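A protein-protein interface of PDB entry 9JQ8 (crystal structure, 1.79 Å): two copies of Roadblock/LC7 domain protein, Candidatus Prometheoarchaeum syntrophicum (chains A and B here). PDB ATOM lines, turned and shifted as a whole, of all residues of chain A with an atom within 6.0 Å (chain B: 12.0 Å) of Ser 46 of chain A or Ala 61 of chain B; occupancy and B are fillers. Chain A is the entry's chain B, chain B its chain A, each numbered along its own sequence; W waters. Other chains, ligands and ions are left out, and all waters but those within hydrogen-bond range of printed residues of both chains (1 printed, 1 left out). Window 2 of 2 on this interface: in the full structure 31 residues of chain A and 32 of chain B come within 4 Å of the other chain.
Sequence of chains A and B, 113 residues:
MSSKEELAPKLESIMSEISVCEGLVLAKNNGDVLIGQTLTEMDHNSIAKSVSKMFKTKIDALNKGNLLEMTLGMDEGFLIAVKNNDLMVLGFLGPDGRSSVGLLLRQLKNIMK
Hydrophobic or aromatic side chains of chain B within 4 Å of the printed part of chain A: Ile 59 and Ala 61.
Printed residues of chain A that touch a printed residue of chain B: Met 42, Ser 46, Ile 47, Ser 50 and Val 51.
Among the printed residues, no Asp or Glu carboxylate lies within 4 Å of a Lys or Arg side-chain nitrogen of the other chain.
Met 42 of chain A touches Leu 62 of chain B (CE to O, 3.7 Å).
Ala 61 of chain B touches Ser 46 of chain A (CB to OG, 3.5 Å).
Ile 47 of chain A touches Ile 59 of chain B (CG2 to CD1, 3.9 Å).
O of Ala 61 of chain B touches CD1 of Ile 47 of chain A (3.4 Å).
Ile 47 of chain A touches Leu 62 of chain B (CD1 to CA, 3.8 Å).
CB of Ser 50 of chain A touches CD1 of Ile 59 of chain B, at 3.7 Å.
CG2 of Val 51 of chain A touches CD1 of Ile 59 of chain B, 3.97 Å away.
Water W1 bridges O of Ala 61 of chain B (2.7 Å) and N of Asp 43 of chain A (2.9 Å).
The backbone carbonyl oxygen (O) of Lys 58 of chain B sits at hydrogen-bond distance from the side-chain hydroxyl (OG) of Ser 50 of chain A.
No position is printed for both chains.
Of the 8 pairs that touch across the chains among the printed residues, none has its exchanged pair printed and touching as well.
Of the printed residues of chain B, Ser 46 of chain A touches Ala 61.
Of chain A, only Ser 46 and Ile 47 come within 4 Å of Ala 61 of chain B.
Met 42 of chain A touches one residue of chain B.
No residue of chain B comes within 4 Å of Asp 43 of chain A.
Ile 47 of chain A touches just these residues of chain B: Ile 59 (3.9 Å), Ala 61 (3.4 Å) and Leu 62 (3.8 Å).
No residue of chain B comes within 4 Å of Ala 48 of chain A.
No residue of chain B comes within 4 Å of Lys 49 of chain A.
Of the printed residues of chain A, Lys 58 of chain B touches Ser 50.
Printed residues of chain A within 4 Å of Ile 59 of chain B: Ile 47 (3.9 Å), Ser 50 (3.7 Å) and Val 51 (3.97 Å).
Of the printed residues of chain B, Val 51 of chain A touches Ile 59 (3.97 Å).
Lys 64 of chain B touches none of the printed residues of chain A.
The backbone carbonyl oxygen (O) of Met 42 of chain A is in hydrogen-bond range of a ring nitrogen (ND1) of His 44 of chain A (3.0 Å).
OD1 of Asp 43 of chain A lies within hydrogen-bond range of N of Ser 46 of chain A.
The backbone carbonyl oxygen (O) of Ser 46 of chain A lies within hydrogen-bond range of the side-chain hydroxyl (OG) of Ser 50 of chain A.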
ATOM      1  N   MET A  42     -23.027  11.307  36.737  1.00  0.00           N
ATOM      2  CA  MET A  42     -23.314  11.896  35.441  1.00  0.00           C
ATOM      3  C   MET A  42     -23.049  10.870  34.356  1.00  0.00           C
ATOM      4  O   MET A  42     -22.204   9.989  34.507  1.00  0.00           O
ATOM      5  CB  MET A  42     -22.475  13.138  35.176  1.00  0.00           C
ATOM      6  CG  MET A  42     -22.478  14.119  36.325  1.00  0.00           C
ATOM      7  SD  MET A  42     -21.820  15.734  35.849  1.00  0.00           S
ATOM      8  CE  MET A  42     -23.017  16.279  34.631  1.00  0.00           C
ATOM      9  N   ASP A  43     -23.782  11.007  33.261  1.00  0.00           N
ATOM     10  CA  ASP A  43     -23.610  10.158  32.085  1.00  0.00           C
ATOM     11  C   ASP A  43     -22.534  10.826  31.236  1.00  0.00           C
ATOM     12  O   ASP A  43     -22.825  11.635  30.351  1.00  0.00           O
ATOM     13  CB  ASP A  43     -24.935  10.022  31.343  1.00  0.00           C
ATOM     14  CG  ASP A  43     -24.849   9.123  30.131  1.00  0.00           C
ATOM     15  OD1 ASP A  43     -23.740   8.689  29.771  1.00  0.00           O
ATOM     16  OD2 ASP A  43     -25.909   8.863  29.532  1.00  0.00           O
ATOM     17  N   HIS A  44     -21.271  10.514  31.535  1.00  0.00           N
ATOM     18  CA  HIS A  44     -20.176  11.173  30.825  1.00  0.00           C
ATOM     19  C   HIS A  44     -20.244  10.876  29.339  1.00  0.00           C
ATOM     20  O   HIS A  44     -19.950  11.744  28.507  1.00  0.00           O
ATOM     21  CB  HIS A  44     -18.808  10.706  31.327  1.00  0.00           C
ATOM     22  CG  HIS A  44     -18.586  10.837  32.805  1.00  0.00           C
ATOM     23  ND1 HIS A  44     -19.563  11.242  33.687  1.00  0.00           N
ATOM     24  CD2 HIS A  44     -17.486  10.578  33.557  1.00  0.00           C
ATOM     25  CE1 HIS A  44     -19.077  11.229  34.918  1.00  0.00           C
ATOM     26  NE2 HIS A  44     -17.818  10.840  34.866  1.00  0.00           N
ATOM     27  N   ASN A  45     -20.563   9.629  28.991  1.00  0.00           N
ATOM     28  CA  ASN A  45     -20.499   9.213  27.596  1.00  0.00           C
ATOM     29  C   ASN A  45     -21.461  10.032  26.750  1.00  0.00           C
ATOM     30  O   ASN A  45     -21.103  10.518  25.675  1.00  0.00           O
ATOM     31  CB  ASN A  45     -20.831   7.727  27.475  1.00  0.00           C
ATOM     32  CG  ASN A  45     -19.700   6.837  27.917  1.00  0.00           C
ATOM     33  OD1 ASN A  45     -18.538   7.187  27.783  1.00  0.00           O
ATOM     34  ND2 ASN A  45     -20.035   5.661  28.430  1.00  0.00           N
ATOM     35  N   SER A  46     -22.693  10.191  27.226  1.00  0.00           N
ATOM     36  CA  SER A  46     -23.683  10.932  26.459  1.00  0.00           C
ATOM     37  C   SER A  46     -23.292  12.397  26.349  1.00  0.00           C
ATOM     38  O   SER A  46     -23.439  13.001  25.284  1.00  0.00           O
ATOM     39  CB  SER A  46     -25.061  10.789  27.105  1.00  0.00           C
ATOM     40  OG  SER A  46     -25.970  11.714  26.543  1.00  0.00           O
ATOM     41  N   ILE A  47     -22.784  12.985  27.433  1.00  0.00           N
ATOM     42  CA  ILE A  47     -22.382  14.388  27.378  1.00  0.00           C
ATOM     43  C   ILE A  47     -21.264  14.584  26.370  1.00  0.00           C
ATOM     44  O   ILE A  47     -21.274  15.543  25.580  1.00  0.00           O
ATOM     45  CB  ILE A  47     -21.967  14.886  28.773  1.00  0.00           C
ATOM     46  CG1 ILE A  47     -23.159  14.874  29.716  1.00  0.00           C
ATOM     47  CG2 ILE A  47     -21.385  16.286  28.673  1.00  0.00           C
ATOM     48  CD1 ILE A  47     -22.784  15.177  31.155  1.00  0.00           C
ATOM     49  N   ALA A  48     -20.267  13.703  26.393  1.00  0.00           N
ATOM     50  CA  ALA A  48     -19.140  13.867  25.480  1.00  0.00           C
ATOM     51  C   ALA A  48     -19.565  13.651  24.029  1.00  0.00           C
ATOM     52  O   ALA A  48     -19.044  14.309  23.118  1.00  0.00           O
ATOM     53  CB  ALA A  48     -18.018  12.910  25.878  1.00  0.00           C
ATOM     54  N   LYS A  49     -20.499  12.724  23.792  1.00  0.00           N
ATOM     55  CA  LYS A  49     -21.017  12.542  22.439  1.00  0.00           C
ATOM     56  C   LYS A  49     -21.659  13.827  21.935  1.00  0.00           C
ATOM     57  O   LYS A  49     -21.436  14.240  20.789  1.00  0.00           O
ATOM     58  CB  LYS A  49     -22.040  11.403  22.403  1.00  0.00           C
ATOM     59  CG  LYS A  49     -21.525  10.025  22.789  1.00  0.00           C
ATOM     60  CD  LYS A  49     -20.236   9.633  22.079  1.00  0.00           C
ATOM     61  CE  LYS A  49     -19.510   8.508  22.863  1.00  0.00           C
ATOM     62  NZ  LYS A  49     -19.104   8.901  24.275  1.00  0.00           N
ATOM     63  N   SER A  50     -22.442  14.486  22.796  1.00  0.00           N
ATOM     64  CA  SER A  50     -23.122  15.725  22.410  1.00  0.00           C
ATOM     65  C   SER A  50     -22.130  16.846  22.136  1.00  0.00           C
ATOM     66  O   SER A  50     -22.282  17.601  21.166  1.00  0.00           O
ATOM     67  CB  SER A  50     -24.093  16.168  23.504  1.00  0.00           C
ATOM     68  OG  SER A  50     -25.151  15.251  23.689  1.00  0.00           O
ATOM     69  N   VAL A  51     -21.116  16.980  22.991  1.00  0.00           N
ATOM     70  CA  VAL A  51     -20.133  18.040  22.811  1.00  0.00           C
ATOM     71  C   VAL A  51     -19.269  17.776  21.583  1.00  0.00           C
ATOM     72  O   VAL A  51     -18.903  18.712  20.856  1.00  0.00           O
ATOM     73  CB  VAL A  51     -19.320  18.189  24.106  1.00  0.00           C
ATOM     74  CG1 VAL A  51     -18.114  19.086  23.928  1.00  0.00           C
ATOM     75  CG2 VAL A  51     -20.247  18.697  25.215  1.00  0.00           C
ATOM     76  N   LYS B  56     -30.197  24.296  19.393  1.00  0.00           N
ATOM     77  CA  LYS B  56     -31.133  23.189  19.563  1.00  0.00           C
ATOM     78  C   LYS B  56     -30.447  21.898  19.986  1.00  0.00           C
ATOM     79  O   LYS B  56     -31.126  20.873  20.139  1.00  0.00           O
ATOM     80  CB  LYS B  56     -31.923  22.955  18.264  1.00  0.00           C
ATOM     81  CG  LYS B  56     -32.938  24.057  17.952  1.00  0.00           C
ATOM     82  CD  LYS B  56     -33.299  24.105  16.464  1.00  0.00           C
ATOM     83  CE  LYS B  56     -34.425  25.113  16.174  1.00  0.00           C
ATOM     84  NZ  LYS B  56     -34.126  26.508  16.641  1.00  0.00           N
ATOM     85  N   THR B  57     -29.129  21.920  20.183  1.00  0.00           N
ATOM     86  CA  THR B  57     -28.413  20.717  20.577  1.00  0.00           C
ATOM     87  C   THR B  57     -28.939  20.207  21.913  1.00  0.00           C
ATOM     88  O   THR B  57     -29.090  20.975  22.866  1.00  0.00           O
ATOM     89  CB  THR B  57     -26.912  20.994  20.688  1.00  0.00           C
ATOM     90  OG1 THR B  57     -26.410  21.477  19.436  1.00  0.00           O
ATOM     91  CG2 THR B  57     -26.178  19.720  21.074  1.00  0.00           C
ATOM     92  N   LYS B  58     -29.233  18.914  21.977  1.00  0.00           N
ATOM     93  CA  LYS B  58     -29.743  18.307  23.198  1.00  0.00           C
ATOM     94  C   LYS B  58     -28.563  17.917  24.074  1.00  0.00           C
ATOM     95  O   LYS B  58     -27.667  17.194  23.628  1.00  0.00           O
ATOM     96  CB  LYS B  58     -30.611  17.089  22.887  1.00  0.00           C
ATOM     97  CG  LYS B  58     -31.920  17.423  22.199  1.00  0.00           C
ATOM     98  CD  LYS B  58     -32.790  16.189  22.055  1.00  0.00           C
ATOM     99  CE  LYS B  58     -34.151  16.532  21.473  1.00  0.00           C
ATOM    100  NZ  LYS B  58     -35.053  15.340  21.438  1.00  0.00           N
ATOM    101  N   ILE B  59     -28.554  18.416  25.305  1.00  0.00           N
ATOM    102  CA  ILE B  59     -27.520  18.064  26.271  1.00  0.00           C
ATOM    103  C   ILE B  59     -28.222  17.867  27.614  1.00  0.00           C
ATOM    104  O   ILE B  59     -27.820  18.419  28.644  1.00  0.00           O
ATOM    105  CB  ILE B  59     -26.403  19.133  26.303  1.00  0.00           C
ATOM    106  CG1 ILE B  59     -25.237  18.739  27.222  1.00  0.00           C
ATOM    107  CG2 ILE B  59     -26.972  20.518  26.631  1.00  0.00           C
ATOM    108  CD1 ILE B  59     -23.981  18.278  26.495  1.00  0.00           C
ATOM    109  N   ASP B  60     -29.303  17.080  27.610  1.00  0.00           N
ATOM    110  CA  ASP B  60     -30.030  16.871  28.856  1.00  0.00           C
ATOM    111  C   ASP B  60     -29.192  16.094  29.856  1.00  0.00           C
ATOM    112  O   ASP B  60     -29.387  16.241  31.066  1.00  0.00           O
ATOM    113  CB  ASP B  60     -31.350  16.140  28.610  1.00  0.00           C
ATOM    114  CG  ASP B  60     -32.230  16.082  29.865  1.00  0.00           C
ATOM    115  OD1 ASP B  60     -31.980  16.851  30.822  1.00  0.00           O
ATOM    116  OD2 ASP B  60     -33.172  15.263  29.899  1.00  0.00           O
ATOM    117  N   ALA B  61     -28.251  15.275  29.376  1.00  0.00           N
ATOM    118  CA  ALA B  61     -27.429  14.490  30.289  1.00  0.00           C
ATOM    119  C   ALA B  61     -26.565  15.388  31.155  1.00  0.00           C
ATOM    120  O   ALA B  61     -26.019  14.935  32.166  1.00  0.00           O
ATOM    121  CB  ALA B  61     -26.558  13.506  29.517  1.00  0.00           C
ATOM    122  N   LEU B  62     -26.427  16.657  30.776  1.00  0.00           N
ATOM    123  CA  LEU B  62     -25.711  17.595  31.617  1.00  0.00           C
ATOM    124  C   LEU B  62     -26.512  17.959  32.860  1.00  0.00           C
ATOM    125  O   LEU B  62     -25.921  18.394  33.854  1.00  0.00           O
ATOM    126  CB  LEU B  62     -25.388  18.843  30.803  1.00  0.00           C
ATOM    127  CG  LEU B  62     -24.457  19.853  31.428  1.00  0.00           C
ATOM    128  CD1 LEU B  62     -23.149  19.166  31.751  1.00  0.00           C
ATOM    129  CD2 LEU B  62     -24.269  20.989  30.440  1.00  0.00           C
ATOM    130  N   ASN B  63     -27.831  17.781  32.822  1.00  0.00           N
ATOM    131  CA  ASN B  63     -28.715  18.073  33.956  1.00  0.00           C
ATOM    132  C   ASN B  63     -28.651  19.546  34.337  1.00  0.00           C
ATOM    133  O   ASN B  63     -28.708  19.902  35.516  1.00  0.00           O
ATOM    134  CB  ASN B  63     -28.387  17.204  35.181  1.00  0.00           C
ATOM    135  CG  ASN B  63     -28.562  15.724  34.924  1.00  0.00           C
ATOM    136  OD1 ASN B  63     -29.408  15.311  34.132  1.00  0.00           O
ATOM    137  ND2 ASN B  63     -27.760  14.912  35.609  1.00  0.00           N
ATOM    138  N   LYS B  64     -28.501  20.418  33.341  1.00  0.00           N
ATOM    139  CA  LYS B  64     -28.420  21.850  33.603  1.00  0.00           C
ATOM    140  C   LYS B  64     -29.494  22.641  32.872  1.00  0.00           C
ATOM    141  O   LYS B  64     -29.403  23.879  32.794  1.00  0.00           O
ATOM    142  CB  LYS B  64     -27.032  22.380  33.227  1.00  0.00           C
ATOM    143  CG  LYS B  64     -25.929  21.860  34.147  1.00  0.00           C
ATOM    144  CD  LYS B  64     -24.633  22.608  33.899  1.00  0.00           C
ATOM    145  CE  LYS B  64     -23.494  22.048  34.774  1.00  0.00           C
ATOM    146  NZ  LYS B  64     -23.775  22.224  36.216  1.00  0.00           N
ATOM    147  N   GLY B  65     -30.519  21.967  32.355  1.00  0.00           N
ATOM    148  CA  GLY B  65     -31.603  22.674  31.699  1.00  0.00           C
ATOM    149  C   GLY B  65     -31.220  23.131  30.302  1.00  0.00           C
ATOM    150  O   GLY B  65     -30.411  22.504  29.612  1.00  0.00           O
ATOM    151  N   ASN B  66     -31.787  24.271  29.903  1.00  0.00           N
ATOM    152  CA  ASN B  66     -31.692  24.757  28.536  1.00  0.00           C
ATOM    153  C   ASN B  66     -30.411  25.546  28.290  1.00  0.00           C
ATOM    154  O   ASN B  66     -29.874  26.206  29.183  1.00  0.00           O
ATOM    155  CB  ASN B  66     -32.889  25.650  28.211  1.00  0.00           C
ATOM    156  CG  ASN B  66     -34.197  24.897  28.232  1.00  0.00           C
ATOM    157  OD1 ASN B  66     -35.158  25.321  28.862  1.00  0.00           O
ATOM    158  ND2 ASN B  66     -34.235  23.757  27.546  1.00  0.00           N
ATOM    159  N   LEU B  67     -29.961  25.497  27.046  1.00  0.00           N
ATOM    160  CA  LEU B  67     -28.801  26.255  26.592  1.00  0.00           C
ATOM    161  C   LEU B  67     -29.230  27.679  26.247  1.00  0.00           C
ATOM    162  O   LEU B  67     -30.106  27.869  25.396  1.00  0.00           O
ATOM    163  CB  LEU B  67     -28.200  25.565  25.373  1.00  0.00           C
ATOM    164  CG  LEU B  67     -27.056  26.255  24.656  1.00  0.00           C
ATOM    165  CD1 LEU B  67     -25.937  26.472  25.652  1.00  0.00           C
ATOM    166  CD2 LEU B  67     -26.601  25.384  23.498  1.00  0.00           C
HETATM  167  O   HOH W   1     -26.210  12.549  33.420  1.00  0.00           O
